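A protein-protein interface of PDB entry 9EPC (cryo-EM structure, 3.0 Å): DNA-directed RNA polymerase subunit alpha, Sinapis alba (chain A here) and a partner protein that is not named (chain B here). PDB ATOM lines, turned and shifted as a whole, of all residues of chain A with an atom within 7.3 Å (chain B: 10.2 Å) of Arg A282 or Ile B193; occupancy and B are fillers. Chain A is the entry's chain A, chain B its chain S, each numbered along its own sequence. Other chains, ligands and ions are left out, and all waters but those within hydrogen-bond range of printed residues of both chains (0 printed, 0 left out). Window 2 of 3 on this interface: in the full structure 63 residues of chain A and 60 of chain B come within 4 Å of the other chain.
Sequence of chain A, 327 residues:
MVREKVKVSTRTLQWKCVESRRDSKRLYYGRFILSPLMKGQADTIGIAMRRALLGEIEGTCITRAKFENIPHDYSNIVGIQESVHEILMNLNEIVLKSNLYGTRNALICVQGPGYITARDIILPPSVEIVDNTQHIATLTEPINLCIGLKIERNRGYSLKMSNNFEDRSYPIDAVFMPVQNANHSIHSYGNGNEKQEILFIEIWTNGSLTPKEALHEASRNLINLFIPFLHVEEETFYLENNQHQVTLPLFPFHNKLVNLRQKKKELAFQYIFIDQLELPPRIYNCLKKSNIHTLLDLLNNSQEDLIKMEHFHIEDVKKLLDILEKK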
ATOM      1  N   LEU A 279     -13.205  26.377   9.654  1.00  0.00           N
ATOM      2  CA  LEU A 279     -13.905  26.205  10.912  1.00  0.00           C
ATOM      3  C   LEU A 279     -13.884  27.496  11.724  1.00  0.00           C
ATOM      4  O   LEU A 279     -13.016  28.350  11.531  1.00  0.00           O
ATOM      5  CB  LEU A 279     -13.268  25.076  11.714  1.00  0.00           C
ATOM      6  CG  LEU A 279     -13.051  23.763  10.964  1.00  0.00           C
ATOM      7  CD1 LEU A 279     -12.489  22.705  11.897  1.00  0.00           C
ATOM      8  CD2 LEU A 279     -14.343  23.288  10.327  1.00  0.00           C
ATOM      9  N   PRO A 280     -14.842  27.667  12.632  1.00  0.00           N
ATOM     10  CA  PRO A 280     -14.783  28.803  13.540  1.00  0.00           C
ATOM     11  C   PRO A 280     -13.552  28.707  14.427  1.00  0.00           C
ATOM     12  O   PRO A 280     -13.061  27.599  14.711  1.00  0.00           O
ATOM     13  CB  PRO A 280     -16.076  28.673  14.356  1.00  0.00           C
ATOM     14  CG  PRO A 280     -16.986  27.879  13.493  1.00  0.00           C
ATOM     15  CD  PRO A 280     -16.102  26.917  12.767  1.00  0.00           C
ATOM     16  N   PRO A 281     -13.015  29.846  14.867  1.00  0.00           N
ATOM     17  CA  PRO A 281     -11.801  29.795  15.699  1.00  0.00           C
ATOM     18  C   PRO A 281     -11.968  28.990  16.976  1.00  0.00           C
ATOM     19  O   PRO A 281     -11.034  28.288  17.381  1.00  0.00           O
ATOM     20  CB  PRO A 281     -11.518  31.276  15.989  1.00  0.00           C
ATOM     21  CG  PRO A 281     -12.827  31.963  15.788  1.00  0.00           C
ATOM     22  CD  PRO A 281     -13.502  31.220  14.680  1.00  0.00           C
ATOM     23  N   ARG A 282     -13.134  29.065  17.624  1.00  0.00           N
ATOM     24  CA  ARG A 282     -13.348  28.266  18.828  1.00  0.00           C
ATOM     25  C   ARG A 282     -13.353  26.778  18.508  1.00  0.00           C
ATOM     26  O   ARG A 282     -12.787  25.975  19.259  1.00  0.00           O
ATOM     27  CB  ARG A 282     -14.653  28.668  19.513  1.00  0.00           C
ATOM     28  CG  ARG A 282     -14.992  27.800  20.718  1.00  0.00           C
ATOM     29  CD  ARG A 282     -16.139  28.369  21.531  1.00  0.00           C
ATOM     30  NE  ARG A 282     -17.373  28.457  20.762  1.00  0.00           N
ATOM     31  CZ  ARG A 282     -18.309  27.519  20.745  1.00  0.00           C
ATOM     32  NH1 ARG A 282     -18.180  26.401  21.440  1.00  0.00           N
ATOM     33  NH2 ARG A 282     -19.402  27.708  20.011  1.00  0.00           N
ATOM     34  N   ILE A 283     -13.986  26.390  17.400  1.00  0.00           N
ATOM     35  CA  ILE A 283     -13.998  24.985  17.006  1.00  0.00           C
ATOM     36  C   ILE A 283     -12.586  24.508  16.708  1.00  0.00           C
ATOM     37  O   ILE A 283     -12.184  23.411  17.117  1.00  0.00           O
ATOM     38  CB  ILE A 283     -14.929  24.778  15.798  1.00  0.00           C
ATOM     39  CG1 ILE A 283     -16.347  25.219  16.149  1.00  0.00           C
ATOM     40  CG2 ILE A 283     -14.912  23.325  15.356  1.00  0.00           C
ATOM     41  CD1 ILE A 283     -16.881  24.560  17.391  1.00  0.00           C
ATOM     42  N   TYR A 284     -11.809  25.322  15.993  1.00  0.00           N
ATOM     43  CA  TYR A 284     -10.453  24.927  15.633  1.00  0.00           C
ATOM     44  C   TYR A 284      -9.579  24.746  16.868  1.00  0.00           C
ATOM     45  O   TYR A 284      -8.816  23.779  16.959  1.00  0.00           O
ATOM     46  CB  TYR A 284      -9.841  25.960  14.691  1.00  0.00           C
ATOM     47  CG  TYR A 284      -8.387  25.709  14.392  1.00  0.00           C
ATOM     48  CD1 TYR A 284      -8.008  24.734  13.485  1.00  0.00           C
ATOM     49  CD2 TYR A 284      -7.392  26.444  15.019  1.00  0.00           C
ATOM     50  CE1 TYR A 284      -6.683  24.498  13.212  1.00  0.00           C
ATOM     51  CE2 TYR A 284      -6.063  26.215  14.751  1.00  0.00           C
ATOM     52  CZ  TYR A 284      -5.714  25.240  13.846  1.00  0.00           C
ATOM     53  OH  TYR A 284      -4.388  25.003  13.570  1.00  0.00           O
ATOM     54  N   ASN A 285      -9.677  25.667  17.829  1.00  0.00           N
ATOM     55  CA  ASN A 285      -8.832  25.582  19.015  1.00  0.00           C
ATOM     56  C   ASN A 285      -9.142  24.337  19.834  1.00  0.00           C
ATOM     57  O   ASN A 285      -8.228  23.672  20.334  1.00  0.00           O
ATOM     58  CB  ASN A 285      -8.995  26.840  19.866  1.00  0.00           C
ATOM     59  CG  ASN A 285      -8.409  28.068  19.202  1.00  0.00           C
ATOM     60  OD1 ASN A 285      -7.516  27.965  18.362  1.00  0.00           O
ATOM     61  ND2 ASN A 285      -8.907  29.238  19.577  1.00  0.00           N
ATOM     62  N   CYS A 286     -10.426  24.004  19.986  1.00  0.00           N
ATOM     63  CA  CYS A 286     -10.792  22.824  20.762  1.00  0.00           C
ATOM     64  C   CYS A 286     -10.282  21.548  20.105  1.00  0.00           C
ATOM     65  O   CYS A 286      -9.771  20.653  20.787  1.00  0.00           O
ATOM     66  CB  CYS A 286     -12.307  22.766  20.944  1.00  0.00           C
ATOM     67  SG  CYS A 286     -12.982  24.153  21.875  1.00  0.00           S
ATOM     68  N   LEU A 287     -10.413  21.445  18.782  1.00  0.00           N
ATOM     69  CA  LEU A 287      -9.926  20.261  18.085  1.00  0.00           C
ATOM     70  C   LEU A 287      -8.415  20.126  18.215  1.00  0.00           C
ATOM     71  O   LEU A 287      -7.898  19.022  18.417  1.00  0.00           O
ATOM     72  CB  LEU A 287     -10.340  20.310  16.617  1.00  0.00           C
ATOM     73  CG  LEU A 287     -11.846  20.258  16.366  1.00  0.00           C
ATOM     74  CD1 LEU A 287     -12.144  20.359  14.884  1.00  0.00           C
ATOM     75  CD2 LEU A 287     -12.432  18.986  16.947  1.00  0.00           C
ATOM     76  N   LYS A 288      -7.689  21.240  18.097  1.00  0.00           N
ATOM     77  CA  LYS A 288      -6.242  21.198  18.276  1.00  0.00           C
ATOM     78  C   LYS A 288      -5.877  20.822  19.704  1.00  0.00           C
ATOM     79  O   LYS A 288      -4.910  20.086  19.932  1.00  0.00           O
ATOM     80  CB  LYS A 288      -5.625  22.545  17.902  1.00  0.00           C
ATOM     81  CG  LYS A 288      -5.789  22.905  16.440  1.00  0.00           C
ATOM     82  CD  LYS A 288      -5.085  21.903  15.550  1.00  0.00           C
ATOM     83  CE  LYS A 288      -3.582  22.042  15.667  1.00  0.00           C
ATOM     84  NZ  LYS A 288      -3.126  23.373  15.187  1.00  0.00           N
ATOM     85  N   MET A 309     -15.523  17.068  25.082  1.00  0.00           N
ATOM     86  CA  MET A 309     -14.480  18.080  25.135  1.00  0.00           C
ATOM     87  C   MET A 309     -14.965  19.298  25.914  1.00  0.00           C
ATOM     88  O   MET A 309     -16.163  19.585  25.980  1.00  0.00           O
ATOM     89  CB  MET A 309     -14.052  18.482  23.725  1.00  0.00           C
ATOM     90  CG  MET A 309     -13.659  17.299  22.854  1.00  0.00           C
ATOM     91  SD  MET A 309     -12.737  17.765  21.378  1.00  0.00           S
ATOM     92  CE  MET A 309     -13.866  18.921  20.618  1.00  0.00           C
ATOM     93  N   HIS A 311     -14.596  22.927  25.939  1.00  0.00           N
ATOM     94  CA  HIS A 311     -15.305  24.055  25.336  1.00  0.00           C
ATOM     95  C   HIS A 311     -16.010  23.653  24.047  1.00  0.00           C
ATOM     96  O   HIS A 311     -15.885  24.306  23.012  1.00  0.00           O
ATOM     97  CB  HIS A 311     -14.339  25.209  25.099  1.00  0.00           C
ATOM     98  CG  HIS A 311     -13.784  25.798  26.356  1.00  0.00           C
ATOM     99  ND1 HIS A 311     -12.633  25.329  26.954  1.00  0.00           N
ATOM    100  CD2 HIS A 311     -14.228  26.811  27.138  1.00  0.00           C
ATOM    101  CE1 HIS A 311     -12.389  26.034  28.045  1.00  0.00           C
ATOM    102  NE2 HIS A 311     -13.341  26.939  28.179  1.00  0.00           N
ATOM    103  N   PHE A 312     -16.781  22.572  24.109  1.00  0.00           N
ATOM    104  CA  PHE A 312     -17.520  22.071  22.961  1.00  0.00           C
ATOM    105  C   PHE A 312     -18.953  21.802  23.388  1.00  0.00           C
ATOM    106  O   PHE A 312     -19.185  21.154  24.413  1.00  0.00           O
ATOM    107  CB  PHE A 312     -16.877  20.800  22.401  1.00  0.00           C
ATOM    108  CG  PHE A 312     -17.171  20.562  20.950  1.00  0.00           C
ATOM    109  CD1 PHE A 312     -16.376  21.127  19.970  1.00  0.00           C
ATOM    110  CD2 PHE A 312     -18.239  19.772  20.567  1.00  0.00           C
ATOM    111  CE1 PHE A 312     -16.637  20.906  18.634  1.00  0.00           C
ATOM    112  CE2 PHE A 312     -18.507  19.550  19.230  1.00  0.00           C
ATOM    113  CZ  PHE A 312     -17.704  20.119  18.263  1.00  0.00           C
ATOM    114  N   HIS A 313     -19.906  22.300  22.610  1.00  0.00           N
ATOM    115  CA  HIS A 313     -21.318  22.204  22.943  1.00  0.00           C
ATOM    116  C   HIS A 313     -22.057  21.406  21.876  1.00  0.00           C
ATOM    117  O   HIS A 313     -21.502  21.042  20.836  1.00  0.00           O
ATOM    118  CB  HIS A 313     -21.942  23.595  23.099  1.00  0.00           C
ATOM    119  CG  HIS A 313     -21.293  24.432  24.158  1.00  0.00           C
ATOM    120  ND1 HIS A 313     -20.463  23.901  25.122  1.00  0.00           N
ATOM    121  CD2 HIS A 313     -21.352  25.762  24.404  1.00  0.00           C
ATOM    122  CE1 HIS A 313     -20.038  24.867  25.915  1.00  0.00           C
ATOM    123  NE2 HIS A 313     -20.563  26.006  25.501  1.00  0.00           N
ATOM    124  N   GLU A 315     -24.617  22.411  20.046  1.00  0.00           N
ATOM    125  CA  GLU A 315     -24.882  23.201  18.848  1.00  0.00           C
ATOM    126  C   GLU A 315     -23.680  23.224  17.914  1.00  0.00           C
ATOM    127  O   GLU A 315     -23.840  23.405  16.701  1.00  0.00           O
ATOM    128  CB  GLU A 315     -25.275  24.630  19.230  1.00  0.00           C
ATOM    129  CG  GLU A 315     -26.459  24.733  20.183  1.00  0.00           C
ATOM    130  CD  GLU A 315     -26.064  24.554  21.637  1.00  0.00           C
ATOM    131  OE1 GLU A 315     -24.868  24.317  21.905  1.00  0.00           O
ATOM    132  OE2 GLU A 315     -26.950  24.650  22.511  1.00  0.00           O
ATOM    133  N   ASP A 316     -22.476  23.040  18.454  1.00  0.00           N
ATOM    134  CA  ASP A 316     -21.273  23.162  17.638  1.00  0.00           C
ATOM    135  C   ASP A 316     -21.081  21.953  16.733  1.00  0.00           C
ATOM    136  O   ASP A 316     -20.609  22.091  15.599  1.00  0.00           O
ATOM    137  CB  ASP A 316     -20.056  23.366  18.534  1.00  0.00           C
ATOM    138  CG  ASP A 316     -20.107  24.677  19.286  1.00  0.00           C
ATOM    139  OD1 ASP A 316     -20.708  24.716  20.380  1.00  0.00           O
ATOM    140  OD2 ASP A 316     -19.563  25.675  18.773  1.00  0.00           O
ATOM    141  N   LYS A 319     -23.090  22.580  13.533  1.00  0.00           N
ATOM    142  CA  LYS A 319     -22.488  23.483  12.558  1.00  0.00           C
ATOM    143  C   LYS A 319     -21.192  22.916  11.999  1.00  0.00           C
ATOM    144  O   LYS A 319     -20.810  23.243  10.871  1.00  0.00           O
ATOM    145  CB  LYS A 319     -22.248  24.859  13.182  1.00  0.00           C
ATOM    146  CG  LYS A 319     -21.198  24.884  14.275  1.00  0.00           C
ATOM    147  CD  LYS A 319     -21.002  26.289  14.815  1.00  0.00           C
ATOM    148  CE  LYS A 319     -22.296  26.842  15.384  1.00  0.00           C
ATOM    149  NZ  LYS A 319     -22.827  25.986  16.480  1.00  0.00           N
ATOM    150  N   GLU B 189     -15.586  42.905  14.899  1.00  0.00           N
ATOM    151  CA  GLU B 189     -15.023  42.041  15.925  1.00  0.00           C
ATOM    152  C   GLU B 189     -15.912  40.811  16.102  1.00  0.00           C
ATOM    153  O   GLU B 189     -16.833  40.563  15.319  1.00  0.00           O
ATOM    154  CB  GLU B 189     -14.852  42.814  17.230  1.00  0.00           C
ATOM    155  CG  GLU B 189     -16.158  43.299  17.837  1.00  0.00           C
ATOM    156  CD  GLU B 189     -15.960  43.974  19.179  1.00  0.00           C
ATOM    157  OE1 GLU B 189     -14.796  44.228  19.552  1.00  0.00           O
ATOM    158  OE2 GLU B 189     -16.970  44.246  19.861  1.00  0.00           O
ATOM    159  N   SER B 190     -15.644  40.026  17.141  1.00  0.00           N
ATOM    160  CA  SER B 190     -16.413  38.821  17.420  1.00  0.00           C
ATOM    161  C   SER B 190     -16.523  38.657  18.933  1.00  0.00           C
ATOM    162  O   SER B 190     -16.225  39.578  19.699  1.00  0.00           O
ATOM    163  CB  SER B 190     -15.771  37.599  16.751  1.00  0.00           C
ATOM    164  OG  SER B 190     -15.739  37.747  15.343  1.00  0.00           O
ATOM    165  N   GLU B 191     -16.958  37.476  19.360  1.00  0.00           N
ATOM    166  CA  GLU B 191     -17.104  37.189  20.779  1.00  0.00           C
ATOM    167  C   GLU B 191     -15.738  37.108  21.454  1.00  0.00           C
ATOM    168  O   GLU B 191     -14.722  36.810  20.819  1.00  0.00           O
ATOM    169  CB  GLU B 191     -17.868  35.879  20.978  1.00  0.00           C
ATOM    170  CG  GLU B 191     -18.307  35.608  22.409  1.00  0.00           C
ATOM    171  CD  GLU B 191     -18.863  34.211  22.594  1.00  0.00           C
ATOM    172  OE1 GLU B 191     -18.867  33.437  21.614  1.00  0.00           O
ATOM    173  OE2 GLU B 191     -19.293  33.884  23.720  1.00  0.00           O
ATOM    174  N   ASP B 192     -15.722  37.380  22.758  1.00  0.00           N
ATOM    175  CA  ASP B 192     -14.499  37.258  23.540  1.00  0.00           C
ATOM    176  C   ASP B 192     -14.150  35.786  23.716  1.00  0.00           C
ATOM    177  O   ASP B 192     -14.643  35.126  24.635  1.00  0.00           O
ATOM    178  CB  ASP B 192     -14.656  37.942  24.899  1.00  0.00           C
ATOM    179  CG  ASP B 192     -13.364  37.971  25.693  1.00  0.00           C
ATOM    180  OD1 ASP B 192     -12.301  37.647  25.123  1.00  0.00           O
ATOM    181  OD2 ASP B 192     -13.413  38.317  26.892  1.00  0.00           O
ATOM    182  N   ILE B 193     -13.298  35.269  22.838  1.00  0.00           N
ATOM    183  CA  ILE B 193     -12.957  33.856  22.821  1.00  0.00           C
ATOM    184  C   ILE B 193     -11.639  33.591  23.557  1.00  0.00           C
ATOM    185  O   ILE B 193     -11.049  32.521  23.413  1.00  0.00           O
ATOM    186  CB  ILE B 193     -12.929  33.316  21.380  1.00  0.00           C
ATOM    187  CG1 ILE B 193     -13.122  31.799  21.358  1.00  0.00           C
ATOM    188  CG2 ILE B 193     -11.657  33.738  20.656  1.00  0.00           C
ATOM    189  CD1 ILE B 193     -14.364  31.355  22.076  1.00  0.00           C
ATOM    190  N   SER B 194     -11.188  34.544  24.376  1.00  0.00           N
ATOM    191  CA  SER B 194      -9.888  34.424  25.028  1.00  0.00           C
ATOM    192  C   SER B 194      -9.810  33.237  25.979  1.00  0.00           C
ATOM    193  O   SER B 194      -8.703  32.801  26.311  1.00  0.00           O
ATOM    194  CB  SER B 194      -9.566  35.711  25.788  1.00  0.00           C
ATOM    195  OG  SER B 194     -10.522  35.949  26.805  1.00  0.00           O
ATOM    196  N   HIS B 195     -10.949  32.704  26.422  1.00  0.00           N
ATOM    197  CA  HIS B 195     -10.929  31.607  27.379  1.00  0.00           C
ATOM    198  C   HIS B 195     -10.352  30.325  26.792  1.00  0.00           C
ATOM    199  O   HIS B 195      -9.857  29.484  27.548  1.00  0.00           O
ATOM    200  CB  HIS B 195     -12.339  31.345  27.910  1.00  0.00           C
ATOM    201  CG  HIS B 195     -13.326  30.977  26.848  1.00  0.00           C
ATOM    202  ND1 HIS B 195     -13.361  29.729  26.264  1.00  0.00           N
ATOM    203  CD2 HIS B 195     -14.314  31.694  26.262  1.00  0.00           C
ATOM    204  CE1 HIS B 195     -14.330  29.693  25.366  1.00  0.00           C
ATOM    205  NE2 HIS B 195     -14.923  30.873  25.345  1.00  0.00           N
ATOM    206  N   THR B 196     -10.403  30.154  25.473  1.00  0.00           N
ATOM    207  CA  THR B 196      -9.902  28.941  24.843  1.00  0.00           C
ATOM    208  C   THR B 196      -8.455  29.057  24.385  1.00  0.00           C
ATOM    209  O   THR B 196      -7.922  28.097  23.819  1.00  0.00           O
ATOM    210  CB  THR B 196     -10.780  28.558  23.648  1.00  0.00           C
ATOM    211  OG1 THR B 196     -10.462  27.225  23.231  1.00  0.00           O
ATOM    212  CG2 THR B 196     -10.540  29.504  22.491  1.00  0.00           C
ATOM    213  N   TYR B 197      -7.807  30.197  24.612  1.00  0.00           N
ATOM    214  CA  TYR B 197      -6.410  30.353  24.223  1.00  0.00           C
ATOM    215  C   TYR B 197      -5.529  29.526  25.149  1.00  0.00           C
ATOM    216  O   TYR B 197      -5.521  29.741  26.365  1.00  0.00           O
ATOM    217  CB  TYR B 197      -6.006  31.824  24.268  1.00  0.00           C
ATOM    218  CG  TYR B 197      -6.750  32.705  23.290  1.00  0.00           C
ATOM    219  CD1 TYR B 197      -7.449  32.159  22.223  1.00  0.00           C
ATOM    220  CD2 TYR B 197      -6.748  34.085  23.434  1.00  0.00           C
ATOM    221  CE1 TYR B 197      -8.128  32.963  21.331  1.00  0.00           C
ATOM    222  CE2 TYR B 197      -7.422  34.895  22.546  1.00  0.00           C
ATOM    223  CZ  TYR B 197      -8.111  34.329  21.498  1.00  0.00           C
ATOM    224  OH  TYR B 197      -8.782  35.136  20.612  1.00  0.00           O
ATOM    225  N   GLY B 198      -4.785  28.587  24.577  1.00  0.00           N
ATOM    226  CA  GLY B 198      -3.980  27.659  25.351  1.00  0.00           C
ATOM    227  C   GLY B 198      -2.514  28.056  25.368  1.00  0.00           C
ATOM    228  O   GLY B 198      -1.967  28.505  24.361  1.00  0.00           O
ATOM    229  N   ARG B 291      -4.298  27.998   9.420  1.00  0.00           N
ATOM    230  CA  ARG B 291      -5.611  28.595   9.222  1.00  0.00           C
ATOM    231  C   ARG B 291      -5.515  30.035   8.741  1.00  0.00           C
ATOM    232  O   ARG B 291      -6.493  30.564   8.204  1.00  0.00           O
ATOM    233  CB  ARG B 291      -6.420  28.531  10.515  1.00  0.00           C
ATOM    234  CG  ARG B 291      -5.702  29.104  11.716  1.00  0.00           C
ATOM    235  CD  ARG B 291      -6.632  29.199  12.905  1.00  0.00           C
ATOM    236  NE  ARG B 291      -5.920  29.587  14.116  1.00  0.00           N
ATOM    237  CZ  ARG B 291      -6.509  29.862  15.271  1.00  0.00           C
ATOM    238  NH1 ARG B 291      -7.824  29.813  15.405  1.00  0.00           N
ATOM    239  NH2 ARG B 291      -5.760  30.197  16.317  1.00  0.00           N
ATOM    240  N   VAL B 334      -7.799  38.012  11.247  1.00  0.00           N
ATOM    241  CA  VAL B 334      -7.748  38.839  12.448  1.00  0.00           C
ATOM    242  C   VAL B 334      -7.898  37.986  13.697  1.00  0.00           C
ATOM    243  O   VAL B 334      -7.291  38.278  14.736  1.00  0.00           O
ATOM    244  CB  VAL B 334      -8.826  39.937  12.379  1.00  0.00           C
ATOM    245  CG1 VAL B 334      -8.716  40.869  13.573  1.00  0.00           C
ATOM    246  CG2 VAL B 334      -8.702  40.711  11.080  1.00  0.00           C
ATOM    247  N   ASP B 335      -8.699  36.922  13.622  1.00  0.00           N
ATOM    248  CA  ASP B 335      -8.859  36.030  14.766  1.00  0.00           C
ATOM    249  C   ASP B 335      -7.528  35.411  15.173  1.00  0.00           C
ATOM    250  O   ASP B 335      -7.250  35.244  16.366  1.00  0.00           O
ATOM    251  CB  ASP B 335      -9.881  34.944  14.440  1.00  0.00           C
ATOM    252  CG  ASP B 335      -9.585  34.247  13.130  1.00  0.00           C
ATOM    253  OD1 ASP B 335      -8.607  34.638  12.458  1.00  0.00           O
ATOM    254  OD2 ASP B 335     -10.328  33.310  12.770  1.00  0.00           O
ATOM    255  N   VAL B 336      -6.693  35.058  14.193  1.00  0.00           N
ATOM    256  CA  VAL B 336      -5.348  34.584  14.502  1.00  0.00           C
ATOM    257  C   VAL B 336      -4.548  35.678  15.194  1.00  0.00           C
ATOM    258  O   VAL B 336      -3.837  35.425  16.173  1.00  0.00           O
ATOM    259  CB  VAL B 336      -4.645  34.091  13.224  1.00  0.00           C
ATOM    260  CG1 VAL B 336      -3.192  33.768  13.510  1.00  0.00           C
ATOM    261  CG2 VAL B 336      -5.359  32.872  12.670  1.00  0.00           C
ATOM    262  N   LEU B 337      -4.657  36.914  14.702  1.00  0.00           N
ATOM    263  CA  LEU B 337      -3.964  38.026  15.340  1.00  0.00           C
ATOM    264  C   LEU B 337      -4.497  38.297  16.739  1.00  0.00           C
ATOM    265  O   LEU B 337      -3.728  38.682  17.627  1.00  0.00           O
ATOM    266  CB  LEU B 337      -4.077  39.279  14.476  1.00  0.00           C
ATOM    267  CG  LEU B 337      -3.380  39.201  13.119  1.00  0.00           C
ATOM    268  CD1 LEU B 337      -3.525  40.509  12.373  1.00  0.00           C
ATOM    269  CD2 LEU B 337      -1.919  38.846  13.302  1.00  0.00           C
ATOM    270  N   LYS B 338      -5.801  38.116  16.957  1.00  0.00           N
ATOM    271  CA  LYS B 338      -6.348  38.282  18.299  1.00  0.00           C
ATOM    272  C   LYS B 338      -5.758  37.262  19.263  1.00  0.00           C
ATOM    273  O   LYS B 338      -5.400  37.601  20.396  1.00  0.00           O
ATOM    274  CB  LYS B 338      -7.871  38.164  18.268  1.00  0.00           C
ATOM    275  CG  LYS B 338      -8.572  39.289  17.532  1.00  0.00           C
ATOM    276  CD  LYS B 338     -10.081  39.120  17.582  1.00  0.00           C
ATOM    277  CE  LYS B 338     -10.788  40.266  16.877  1.00  0.00           C
ATOM    278  NZ  LYS B 338     -12.268  40.118  16.920  1.00  0.00           N
ATOM    279  N   GLU B 339      -5.650  36.006  18.830  1.00  0.00           N
ATOM    280  CA  GLU B 339      -5.104  34.971  19.701  1.00  0.00           C
ATOM    281  C   GLU B 339      -3.606  35.150  19.905  1.00  0.00           C
ATOM    282  O   GLU B 339      -3.103  34.988  21.022  1.00  0.00           O
ATOM    283  CB  GLU B 339      -5.402  33.589  19.123  1.00  0.00           C
ATOM    284  CG  GLU B 339      -4.799  32.446  19.922  1.00  0.00           C
ATOM    285  CD  GLU B 339      -5.207  31.089  19.390  1.00  0.00           C
ATOM    286  OE1 GLU B 339      -5.992  31.043  18.421  1.00  0.00           O
ATOM    287  OE2 GLU B 339      -4.745  30.068  19.941  1.00  0.00           O
ATOM    288  N   ALA B 340      -2.880  35.485  18.841  1.00  0.00           N
ATOM    289  CA  ALA B 340      -1.432  35.594  18.928  1.00  0.00           C
ATOM    290  C   ALA B 340      -1.029  36.731  19.857  1.00  0.00           C
ATOM    291  O   ALA B 340      -1.606  37.820  19.820  1.00  0.00           O
ATOM    292  CB  ALA B 340      -0.835  35.814  17.540  1.00  0.00           C
ATOM    293  N   LYS B 341      -0.036  36.467  20.700  1.00  0.00           N
ATOM    294  CA  LYS B 341       0.539  37.482  21.569  1.00  0.00           C
ATOM    295  C   LYS B 341       1.847  38.039  21.034  1.00  0.00           C
ATOM    296  O   LYS B 341       2.470  38.870  21.701  1.00  0.00           O
ATOM    297  CB  LYS B 341       0.754  36.918  22.975  1.00  0.00           C
ATOM    298  CG  LYS B 341      -0.531  36.590  23.705  1.00  0.00           C
ATOM    299  CD  LYS B 341      -1.419  37.814  23.808  1.00  0.00           C
ATOM    300  CE  LYS B 341      -2.737  37.482  24.481  1.00  0.00           C
ATOM    301  NZ  LYS B 341      -3.632  38.669  24.538  1.00  0.00           N
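Hydrophobic or aromatic side chains of chain B within 4 Å of the printed part of chain A: Ile B193 and His B195. Among the printed residues, 8 pairs touch across the chains.
Pro A281 touches Arg B291. Asp B335 touches Pro A281. Arg A282 touches Ile B193 (CD to CD1, 3.5 Å). Arg B291 touches Tyr A284 (NH1 to CD2, 3.4 Å). Asn A285 touches Thr B196 (ND2 to CG2, 3.4 Å).
SG of Cys A286 lies within hydrogen-bond range of O of His A311, 3.1 Å away. The guanidinium group of Arg A282 lies within salt-bridge range of the side-chain carboxylate of Asp A316 (3.1 Å). The guanidinium group (NH1) of Arg B291 is in salt-bridge range of the side-chain carboxylate (OE1) of Glu B339 (3.7 Å). O of Arg A282 is in hydrogen-bond range of SG of Cys A286, at 3.2 Å. NH1 of Arg A282 sits at hydrogen-bond distance from O of His A311, at 3.5 Å. O of Pro A281 is in hydrogen-bond range of ND2 of Asn A285, 3.2 Å away.
Of chain B, only Ile B193 comes within 4 Å of Arg A282. Printed residues of chain B within 4 Å of Tyr A284: Arg B291 (3.4 Å). Of chain B, only Thr B196 (3.4 Å), Arg B291 (3.5 Å) and Glu B339 (3.4 Å) come within 4 Å of Asn A285. Printed residues of chain B within 4 Å of His A311: His B195 (3.2 Å). Asp A316 touches none of the printed residues of chain B. Of chain A, only Arg A282 comes within 4 Å of Ile B193. Printed residues of chain A within 4 Å of His B195: His A311. Printed residues of chain A within 4 Å of Thr B196: Asn A285 (3.4 Å). Gly B198 touches none of the printed residues of chain A. The nearest residue of chain B that does not touch Arg A282 is His B195 (4.4 Å). The nearest residue of chain A that does not touch Ile B193 is Asn A285 (5.2 Å).
A ring nitrogen (ND1) of His B195 sits close to a ring nitrogen (NE2) of His A311, at 3.4 Å. OD1 of Asn A285 lies within hydrogen-bond range of NH2 of Arg B291, at 3.5 Å. The side-chain carboxylate (OE1) of Glu B339 sits close to the side-chain amide oxygen (OD1) of Asn A285.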
